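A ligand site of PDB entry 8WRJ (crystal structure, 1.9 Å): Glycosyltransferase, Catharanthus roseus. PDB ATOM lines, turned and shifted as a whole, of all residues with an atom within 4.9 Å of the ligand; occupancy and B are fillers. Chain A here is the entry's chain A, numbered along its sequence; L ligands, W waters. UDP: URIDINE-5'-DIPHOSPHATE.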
ATOM      1  N   LYS A  23      15.820   0.550  -5.416  1.00  0.00           N
ATOM      2  CA  LYS A  23      16.277   1.599  -4.507  1.00  0.00           C
ATOM      3  C   LYS A  23      15.897   1.320  -3.057  1.00  0.00           C
ATOM      4  O   LYS A  23      16.669   1.632  -2.140  1.00  0.00           O
ATOM      5  CB  LYS A  23      15.741   2.966  -4.972  1.00  0.00           C
ATOM      6  CG  LYS A  23      16.474   3.414  -6.247  1.00  0.00           C
ATOM      7  CD  LYS A  23      16.188   4.837  -6.663  1.00  0.00           C
ATOM      8  CE  LYS A  23      16.918   5.179  -7.979  1.00  0.00           C
ATOM      9  NZ  LYS A  23      16.973   4.041  -8.924  1.00  0.00           N
ATOM     10  N   GLY A  24      14.733   0.713  -2.815  1.00  0.00           N
ATOM     11  CA  GLY A  24      14.355   0.364  -1.451  1.00  0.00           C
ATOM     12  C   GLY A  24      15.169  -0.782  -0.851  1.00  0.00           C
ATOM     13  O   GLY A  24      15.044  -1.056   0.348  1.00  0.00           O
ATOM     14  N   ASN A  27      19.281   1.365  -0.886  1.00  0.00           N
ATOM     15  CA  ASN A  27      19.495   2.472   0.038  1.00  0.00           C
ATOM     16  C   ASN A  27      19.697   2.026   1.488  1.00  0.00           C
ATOM     17  O   ASN A  27      20.660   2.504   2.119  1.00  0.00           O
ATOM     18  CB  ASN A  27      18.350   3.500  -0.100  1.00  0.00           C
ATOM     19  CG  ASN A  27      18.414   4.285  -1.406  1.00  0.00           C
ATOM     20  OD1 ASN A  27      19.385   4.209  -2.154  1.00  0.00           O
ATOM     21  ND2 ASN A  27      17.348   5.026  -1.708  1.00  0.00           N
ATOM     22  N   TYR A 268      23.481   9.616  -0.709  1.00  0.00           N
ATOM     23  CA  TYR A 268      22.700   9.222  -1.872  1.00  0.00           C
ATOM     24  C   TYR A 268      23.621   8.842  -3.027  1.00  0.00           C
ATOM     25  O   TYR A 268      24.686   9.443  -3.209  1.00  0.00           O
ATOM     26  CB  TYR A 268      21.735  10.340  -2.338  1.00  0.00           C
ATOM     27  CG  TYR A 268      20.919  11.012  -1.226  1.00  0.00           C
ATOM     28  CD1 TYR A 268      19.819  10.365  -0.644  1.00  0.00           C
ATOM     29  CD2 TYR A 268      21.230  12.292  -0.771  1.00  0.00           C
ATOM     30  CE1 TYR A 268      19.065  10.975   0.377  1.00  0.00           C
ATOM     31  CE2 TYR A 268      20.487  12.912   0.236  1.00  0.00           C
ATOM     32  CZ  TYR A 268      19.399  12.239   0.812  1.00  0.00           C
ATOM     33  OH  TYR A 268      18.652  12.882   1.803  1.00  0.00           O
ATOM     34  N   THR A 272      19.364  13.418  -6.704  1.00  0.00           N
ATOM     35  CA  THR A 272      18.325  13.775  -5.744  1.00  0.00           C
ATOM     36  C   THR A 272      17.874  15.219  -5.834  1.00  0.00           C
ATOM     37  O   THR A 272      16.991  15.607  -5.058  1.00  0.00           O
ATOM     38  CB  THR A 272      18.804  13.518  -4.310  1.00  0.00           C
ATOM     39  OG1 THR A 272      20.036  14.222  -4.106  1.00  0.00           O
ATOM     40  CG2 THR A 272      19.008  12.003  -4.061  1.00  0.00           C
ATOM     41  N   TYR A 291       4.701  16.567   2.074  1.00  0.00           N
ATOM     42  CA  TYR A 291       5.610  15.812   1.211  1.00  0.00           C
ATOM     43  C   TYR A 291       4.855  14.625   0.633  1.00  0.00           C
ATOM     44  O   TYR A 291       4.141  13.920   1.358  1.00  0.00           O
ATOM     45  CB  TYR A 291       6.842  15.366   2.007  1.00  0.00           C
ATOM     46  CG  TYR A 291       7.771  14.462   1.237  1.00  0.00           C
ATOM     47  CD1 TYR A 291       8.148  14.750  -0.066  1.00  0.00           C
ATOM     48  CD2 TYR A 291       8.289  13.305   1.838  1.00  0.00           C
ATOM     49  CE1 TYR A 291       9.028  13.897  -0.771  1.00  0.00           C
ATOM     50  CE2 TYR A 291       9.125  12.461   1.147  1.00  0.00           C
ATOM     51  CZ  TYR A 291       9.504  12.747  -0.142  1.00  0.00           C
ATOM     52  OH  TYR A 291      10.356  11.858  -0.807  1.00  0.00           O
ATOM     53  N   SER A 293       5.116  11.181  -1.986  1.00  0.00           N
ATOM     54  CA  SER A 293       5.950  10.292  -2.780  1.00  0.00           C
ATOM     55  C   SER A 293       5.425   8.868  -2.711  1.00  0.00           C
ATOM     56  O   SER A 293       5.039   8.388  -1.624  1.00  0.00           O
ATOM     57  CB  SER A 293       7.417  10.330  -2.315  1.00  0.00           C
ATOM     58  OG  SER A 293       8.156   9.303  -2.972  1.00  0.00           O
ATOM     59  N   GLY A 295       7.438   6.370  -3.826  1.00  0.00           N
ATOM     60  CA  GLY A 295       8.613   5.529  -3.830  1.00  0.00           C
ATOM     61  C   GLY A 295       9.249   5.381  -5.207  1.00  0.00           C
ATOM     62  O   GLY A 295       9.059   6.192  -6.111  1.00  0.00           O
ATOM     63  N   SER A 296      10.028   4.303  -5.335  1.00  0.00           N
ATOM     64  CA  SER A 296      10.884   4.099  -6.501  1.00  0.00           C
ATOM     65  C   SER A 296      10.263   3.186  -7.555  1.00  0.00           C
ATOM     66  O   SER A 296      10.755   3.157  -8.684  1.00  0.00           O
ATOM     67  CB  SER A 296      12.247   3.496  -6.059  1.00  0.00           C
ATOM     68  OG  SER A 296      12.109   2.127  -5.703  1.00  0.00           O
ATOM     69  N   LEU A 297       9.203   2.470  -7.215  1.00  0.00           N
ATOM     70  CA  LEU A 297       8.653   1.402  -8.052  1.00  0.00           C
ATOM     71  C   LEU A 297       7.194   1.587  -8.425  1.00  0.00           C
ATOM     72  O   LEU A 297       6.815   1.321  -9.571  1.00  0.00           O
ATOM     73  CB  LEU A 297       8.800   0.058  -7.353  1.00  0.00           C
ATOM     74  CG  LEU A 297      10.218  -0.425  -7.105  1.00  0.00           C
ATOM     75  CD1 LEU A 297      10.186  -1.693  -6.285  1.00  0.00           C
ATOM     76  CD2 LEU A 297      10.934  -0.637  -8.430  1.00  0.00           C
ATOM     77  N   VAL A 322       7.155  14.127  -5.338  1.00  0.00           N
ATOM     78  CA  VAL A 322       8.062  13.359  -6.196  1.00  0.00           C
ATOM     79  C   VAL A 322       7.236  12.601  -7.228  1.00  0.00           C
ATOM     80  O   VAL A 322       6.510  11.660  -6.879  1.00  0.00           O
ATOM     81  CB  VAL A 322       8.944  12.413  -5.385  1.00  0.00           C
ATOM     82  CG1 VAL A 322       9.805  11.560  -6.319  1.00  0.00           C
ATOM     83  CG2 VAL A 322       9.821  13.194  -4.441  1.00  0.00           C
ATOM     84  N   TRP A 349      12.856  13.428  -8.239  1.00  0.00           N
ATOM     85  CA  TRP A 349      13.483  12.729  -7.129  1.00  0.00           C
ATOM     86  C   TRP A 349      13.999  13.787  -6.181  1.00  0.00           C
ATOM     87  O   TRP A 349      14.434  14.846  -6.628  1.00  0.00           O
ATOM     88  CB  TRP A 349      14.639  11.821  -7.606  1.00  0.00           C
ATOM     89  CG  TRP A 349      14.927  10.577  -6.744  1.00  0.00           C
ATOM     90  CD1 TRP A 349      16.102  10.273  -6.088  1.00  0.00           C
ATOM     91  CD2 TRP A 349      14.030   9.489  -6.470  1.00  0.00           C
ATOM     92  NE1 TRP A 349      15.982   9.049  -5.439  1.00  0.00           N
ATOM     93  CE2 TRP A 349      14.725   8.553  -5.658  1.00  0.00           C
ATOM     94  CE3 TRP A 349      12.706   9.215  -6.843  1.00  0.00           C
ATOM     95  CZ2 TRP A 349      14.129   7.389  -5.206  1.00  0.00           C
ATOM     96  CZ3 TRP A 349      12.129   8.029  -6.404  1.00  0.00           C
ATOM     97  CH2 TRP A 349      12.839   7.142  -5.577  1.00  0.00           C
ATOM     98  N   CYS A 350      13.963  13.511  -4.884  1.00  0.00           N
ATOM     99  CA  CYS A 350      14.342  14.481  -3.858  1.00  0.00           C
ATOM    100  C   CYS A 350      15.306  13.816  -2.901  1.00  0.00           C
ATOM    101  O   CYS A 350      15.494  12.594  -2.949  1.00  0.00           O
ATOM    102  CB  CYS A 350      13.090  14.989  -3.113  1.00  0.00           C
ATOM    103  SG  CYS A 350      12.433  13.919  -1.805  1.00  0.00           S
ATOM    104  N   PRO A 351      15.984  14.582  -2.068  1.00  0.00           N
ATOM    105  CA  PRO A 351      16.802  13.957  -1.015  1.00  0.00           C
ATOM    106  C   PRO A 351      15.922  13.595   0.169  1.00  0.00           C
ATOM    107  O   PRO A 351      15.760  14.411   1.093  1.00  0.00           O
ATOM    108  CB  PRO A 351      17.828  15.041  -0.674  1.00  0.00           C
ATOM    109  CG  PRO A 351      17.060  16.339  -0.911  1.00  0.00           C
ATOM    110  CD  PRO A 351      16.101  16.064  -2.039  1.00  0.00           C
ATOM    111  N   GLN A 352      15.329  12.397   0.157  1.00  0.00           N
ATOM    112  CA  GLN A 352      14.178  12.157   1.032  1.00  0.00           C
ATOM    113  C   GLN A 352      14.530  12.296   2.504  1.00  0.00           C
ATOM    114  O   GLN A 352      13.712  12.792   3.300  1.00  0.00           O
ATOM    115  CB  GLN A 352      13.565  10.773   0.756  1.00  0.00           C
ATOM    116  CG  GLN A 352      12.530  10.371   1.833  1.00  0.00           C
ATOM    117  CD  GLN A 352      11.561   9.312   1.368  1.00  0.00           C
ATOM    118  OE1 GLN A 352      11.359   8.299   2.059  1.00  0.00           O
ATOM    119  NE2 GLN A 352      10.968   9.518   0.197  1.00  0.00           N
ATOM    120  N   LEU A 353      15.723  11.855   2.914  1.00  0.00           N
ATOM    121  CA  LEU A 353      16.109  12.017   4.315  1.00  0.00           C
ATOM    122  C   LEU A 353      16.145  13.497   4.707  1.00  0.00           C
ATOM    123  O   LEU A 353      15.677  13.869   5.790  1.00  0.00           O
ATOM    124  CB  LEU A 353      17.480  11.392   4.577  1.00  0.00           C
ATOM    125  CG  LEU A 353      17.626   9.900   4.236  1.00  0.00           C
ATOM    126  CD1 LEU A 353      19.029   9.420   4.631  1.00  0.00           C
ATOM    127  CD2 LEU A 353      16.573   9.082   4.918  1.00  0.00           C
ATOM    128  N   HIS A 367       3.253   5.856  -0.066  1.00  0.00           N
ATOM    129  CA  HIS A 367       2.809   4.512  -0.396  1.00  0.00           C
ATOM    130  C   HIS A 367       3.120   3.497   0.703  1.00  0.00           C
ATOM    131  O   HIS A 367       2.708   2.347   0.581  1.00  0.00           O
ATOM    132  CB  HIS A 367       3.425   4.044  -1.723  1.00  0.00           C
ATOM    133  CG  HIS A 367       4.856   3.626  -1.623  1.00  0.00           C
ATOM    134  ND1 HIS A 367       5.831   4.437  -1.067  1.00  0.00           N
ATOM    135  CD2 HIS A 367       5.495   2.504  -2.048  1.00  0.00           C
ATOM    136  CE1 HIS A 367       7.001   3.812  -1.123  1.00  0.00           C
ATOM    137  NE2 HIS A 367       6.823   2.642  -1.716  1.00  0.00           N
ATOM    138  N   GLY A 369       6.004   2.147   1.650  1.00  0.00           N
ATOM    139  CA  GLY A 369       7.172   1.273   1.577  1.00  0.00           C
ATOM    140  C   GLY A 369       7.922   1.340   2.891  1.00  0.00           C
ATOM    141  O   GLY A 369       7.816   2.323   3.624  1.00  0.00           O
ATOM    142  N   TRP A 370       8.659   0.278   3.226  1.00  0.00           N
ATOM    143  CA  TRP A 370       9.226   0.223   4.573  1.00  0.00           C
ATOM    144  C   TRP A 370      10.232   1.328   4.826  1.00  0.00           C
ATOM    145  O   TRP A 370      10.242   1.916   5.913  1.00  0.00           O
ATOM    146  CB  TRP A 370       9.874  -1.137   4.861  1.00  0.00           C
ATOM    147  CG  TRP A 370      10.485  -1.121   6.246  1.00  0.00           C
ATOM    148  CD1 TRP A 370      11.770  -1.369   6.567  1.00  0.00           C
ATOM    149  CD2 TRP A 370       9.819  -0.807   7.491  1.00  0.00           C
ATOM    150  NE1 TRP A 370      11.965  -1.268   7.919  1.00  0.00           N
ATOM    151  CE2 TRP A 370      10.783  -0.905   8.512  1.00  0.00           C
ATOM    152  CE3 TRP A 370       8.490  -0.470   7.835  1.00  0.00           C
ATOM    153  CZ2 TRP A 370      10.472  -0.678   9.855  1.00  0.00           C
ATOM    154  CZ3 TRP A 370       8.186  -0.228   9.180  1.00  0.00           C
ATOM    155  CH2 TRP A 370       9.180  -0.338  10.174  1.00  0.00           C
ATOM    156  N   ASN A 371      11.099   1.643   3.859  1.00  0.00           N
ATOM    157  CA  ASN A 371      12.084   2.695   4.104  1.00  0.00           C
ATOM    158  C   ASN A 371      11.386   4.039   4.339  1.00  0.00           C
ATOM    159  O   ASN A 371      11.787   4.790   5.227  1.00  0.00           O
ATOM    160  CB  ASN A 371      13.039   2.815   2.939  1.00  0.00           C
ATOM    161  CG  ASN A 371      13.902   1.601   2.790  1.00  0.00           C
ATOM    162  OD1 ASN A 371      14.828   1.369   3.580  1.00  0.00           O
ATOM    163  ND2 ASN A 371      13.561   0.762   1.821  1.00  0.00           N
ATOM    164  N   SER A 372      10.371   4.353   3.545  1.00  0.00           N
ATOM    165  CA  SER A 372       9.710   5.641   3.759  1.00  0.00           C
ATOM    166  C   SER A 372       8.983   5.685   5.097  1.00  0.00           C
ATOM    167  O   SER A 372       8.986   6.718   5.792  1.00  0.00           O
ATOM    168  CB  SER A 372       8.738   5.907   2.597  1.00  0.00           C
ATOM    169  OG  SER A 372       9.456   6.199   1.410  1.00  0.00           O
ATOM    170  N   GLU A 375      11.789   5.963   7.801  1.00  0.00           N
ATOM    171  CA  GLU A 375      12.435   7.274   7.741  1.00  0.00           C
ATOM    172  C   GLU A 375      11.511   8.366   8.264  1.00  0.00           C
ATOM    173  O   GLU A 375      11.951   9.271   8.981  1.00  0.00           O
ATOM    174  CB  GLU A 375      12.875   7.591   6.306  1.00  0.00           C
ATOM    175  CG  GLU A 375      14.072   6.713   5.838  1.00  0.00           C
ATOM    176  CD  GLU A 375      14.257   6.624   4.325  1.00  0.00           C
ATOM    177  OE1 GLU A 375      13.617   7.407   3.601  1.00  0.00           O
ATOM    178  OE2 GLU A 375      15.060   5.757   3.850  1.00  0.00           O
ATOM    179  N   TRP A 389       0.956  -2.164  -2.784  1.00  0.00           N
ATOM    180  CA  TRP A 389       1.099  -3.613  -2.886  1.00  0.00           C
ATOM    181  C   TRP A 389       2.211  -4.086  -1.944  1.00  0.00           C
ATOM    182  O   TRP A 389       2.807  -3.302  -1.209  1.00  0.00           O
ATOM    183  CB  TRP A 389       1.374  -4.037  -4.342  1.00  0.00           C
ATOM    184  CG  TRP A 389       2.204  -3.063  -5.129  1.00  0.00           C
ATOM    185  CD1 TRP A 389       1.770  -2.226  -6.126  1.00  0.00           C
ATOM    186  CD2 TRP A 389       3.623  -2.859  -5.026  1.00  0.00           C
ATOM    187  NE1 TRP A 389       2.829  -1.493  -6.629  1.00  0.00           N
ATOM    188  CE2 TRP A 389       3.976  -1.869  -5.969  1.00  0.00           C
ATOM    189  CE3 TRP A 389       4.618  -3.416  -4.218  1.00  0.00           C
ATOM    190  CZ2 TRP A 389       5.294  -1.424  -6.121  1.00  0.00           C
ATOM    191  CZ3 TRP A 389       5.929  -2.972  -4.376  1.00  0.00           C
ATOM    192  CH2 TRP A 389       6.252  -1.987  -5.317  1.00  0.00           C
ATOM    193  N   GLN A 392       3.436  -2.906   1.751  1.00  0.00           N
ATOM    194  CA  GLN A 392       2.890  -1.566   1.991  1.00  0.00           C
ATOM    195  C   GLN A 392       1.525  -1.638   2.674  1.00  0.00           C
ATOM    196  O   GLN A 392       1.190  -0.779   3.488  1.00  0.00           O
ATOM    197  CB  GLN A 392       2.785  -0.808   0.677  1.00  0.00           C
ATOM    198  CG  GLN A 392       4.109  -0.545  -0.031  1.00  0.00           C
ATOM    199  CD  GLN A 392       3.933  -0.498  -1.530  1.00  0.00           C
ATOM    200  OE1 GLN A 392       2.856  -0.163  -2.016  1.00  0.00           O
ATOM    201  NE2 GLN A 392       4.975  -0.872  -2.270  1.00  0.00           N
HETATM  202  N1  UDP L   1      13.692   8.160  -1.981  1.00  0.00           N
HETATM  203  C2  UDP L   1      14.450   9.194  -2.272  1.00  0.00           C
HETATM  204  N3  UDP L   1      13.994  10.241  -2.951  1.00  0.00           N
HETATM  205  C4  UDP L   1      12.725  10.237  -3.337  1.00  0.00           C
HETATM  206  C5  UDP L   1      11.889   9.168  -3.059  1.00  0.00           C
HETATM  207  C6  UDP L   1      12.422   8.095  -2.349  1.00  0.00           C
HETATM  208  O2  UDP L   1      15.789   9.203  -1.857  1.00  0.00           O
HETATM  209  O4  UDP L   1      12.241  11.322  -4.042  1.00  0.00           O
HETATM  210  C1' UDP L   1      14.270   6.997  -1.279  1.00  0.00           C
HETATM  211  C2' UDP L   1      13.684   6.764   0.122  1.00  0.00           C
HETATM  212  O2' UDP L   1      14.474   7.419   1.029  1.00  0.00           O
HETATM  213  C3' UDP L   1      13.813   5.222   0.236  1.00  0.00           C
HETATM  214  C4' UDP L   1      13.630   4.739  -0.979  1.00  0.00           C
HETATM  215  O4' UDP L   1      13.943   5.932  -1.996  1.00  0.00           O
HETATM  216  O3' UDP L   1      15.224   4.928   0.586  1.00  0.00           O
HETATM  217  C5' UDP L   1      12.222   4.228  -1.214  1.00  0.00           C
HETATM  218  O5' UDP L   1      12.136   3.033  -0.476  1.00  0.00           O
HETATM  219  PA  UDP L   1      10.697   2.475   0.079  1.00  0.00           P
HETATM  220  O1A UDP L   1      10.866   1.234   0.919  1.00  0.00           O
HETATM  221  O2A UDP L   1       9.960   3.578   0.802  1.00  0.00           O
HETATM  222  O3A UDP L   1       9.711   2.139  -1.181  1.00  0.00           O
HETATM  223  PB  UDP L   1      10.029   1.365  -2.570  1.00  0.00           P
HETATM  224  O1B UDP L   1      10.911   0.154  -2.315  1.00  0.00           O
HETATM  225  O2B UDP L   1      10.616   2.314  -3.568  1.00  0.00           O
HETATM  226  O3B UDP L   1       8.679   0.858  -3.028  1.00  0.00           O
HETATM  227  O   HOH W   1      16.897   8.510   0.686  1.00  0.00           O
HETATM  228  O   HOH W   2      17.625   7.566  -3.348  1.00  0.00           O
HETATM  229  O   HOH W   3       9.443   7.719  -1.102  1.00  0.00           O
HETATM  230  O   HOH W   4      12.700  -0.815  -4.058  1.00  0.00           O
HETATM  231  O   HOH W   5       7.402   2.248  -4.928  1.00  0.00           O
HETATM  232  O   HOH W   6       7.615  -1.233  -1.326  1.00  0.00           O
HETATM  233  O   HOH W   7      17.130   6.121   2.286  1.00  0.00           O
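An oxygen (O2B) of the ligand sits at hydrogen-bond distance from the backbone NH of Ser 296, 2.7 Å away.
The side-chain hydroxyl of Ser 296 sits at hydrogen-bond distance from an oxygen (O2B) of the ligand.
An oxygen (O2') of the ligand lies within hydrogen-bond range of the side-chain carboxylate (OE1) of Glu 375.
N of Ser 372 lies within hydrogen-bond range of O2A of the ligand, at 2.9 Å.
OG of Ser 372 sits at hydrogen-bond distance from O2A of the ligand (2.7 Å).
The backbone NH of Cys 350 lies within hydrogen-bond range of an oxygen (O4) of the ligand (2.9 Å).
O of Cys 350 sits at hydrogen-bond distance from N3 of the ligand, 2.8 Å away.
O4 of the ligand lies within hydrogen-bond range of SG of Cys 350.
An oxygen (O1A) of the ligand sits at hydrogen-bond distance from the backbone NH (N) of Asn 371, 3.0 Å away.
ND2 of Asn 371 sits at hydrogen-bond distance from O1A of the ligand, 2.9 Å away.
NE2 of His 367 is in hydrogen-bond range of O3B of the ligand (2.9 Å).
The side-chain amide nitrogen (ND2) of Asn 27 lies within hydrogen-bond range of an oxygen (O3') of the ligand (3.1 Å).
An oxygen (O2') of the ligand lies close to the side-chain amide oxygen of Gln 352, 3.4 Å away.
N of Trp 370 sits at hydrogen-bond distance from O1A of the ligand (3.3 Å).
The indole nitrogen (NE1) of Trp 349 sits close to a nitrogen (N3) of the ligand.
Gly 24 touches the ligand.
Tyr 291 touches the ligand (OH to O4, 3.8 Å).
Ser 293 touches the ligand.
Gly 295 touches the ligand.
N of Leu 297 touches O2B of the ligand, 3.9 Å away.
Val 322 touches the ligand.
Gly 369 touches the ligand.
Hydrophobic or aromatic side chains within 4 Å of the ligand: Val 322, Trp 349 and His 367.
The nearest printed residue that does not touch the ligand is Gln 392 (4.2 Å).
Water W5 lies within hydrogen-bond range of O3B of the ligand (2.7 Å), N of Leu 297 (2.9 Å), NE2 of His 367 (3.3 Å) and N of Ser 296 (3.4 Å).
Water W4 lies within hydrogen-bond range of O1B of the ligand, N of Gly 24 and OG of Ser 296.
Water W7 bridges the side-chain carboxylate of Glu 375 (2.6 Å) and an oxygen (O3') of the ligand (2.8 Å).
Water W2 lies within hydrogen-bond range of O2 of the ligand (2.9 Å), ND2 of Asn 27 (3.0 Å) and NE1 of Trp 349 (3.0 Å).
Water W6 lies within hydrogen-bond range of NE2 of Gln 392 (2.8 Å) and O3B of the ligand (2.9 Å).
Water W3 lies within hydrogen-bond range of the side-chain amide nitrogen (NE2) of Gln 352, the side-chain hydroxyl (OG) of Ser 293 and the side-chain hydroxyl (OG) of Ser 372.
OE1 of Gln 352 lies close to OE1 of Glu 375 (2.9 Å).
OE1 of Gln 352 lies within hydrogen-bond range of OG of Ser 372, 2.9 Å away.
The side-chain sulfur (SG) of Cys 350 lies within hydrogen-bond range of the side-chain hydroxyl (OH) of Tyr 291, at 3.1 Å.
The backbone carbonyl oxygen of Gly 24 sits at hydrogen-bond distance from the side-chain amide nitrogen of Asn 371.
O of Ser 293 is in hydrogen-bond range of N of His 367 (3.5 Å).
ND2 of Asn 27 sits close to O of Lys 23.
The side-chain hydroxyl of Tyr 291 lies within hydrogen-bond range of the side-chain amide nitrogen of Gln 352, at 2.6 Å.
The backbone NH (N) of Gly 295 is in hydrogen-bond range of the side-chain hydroxyl (OG) of Ser 293, 3.1 Å away.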
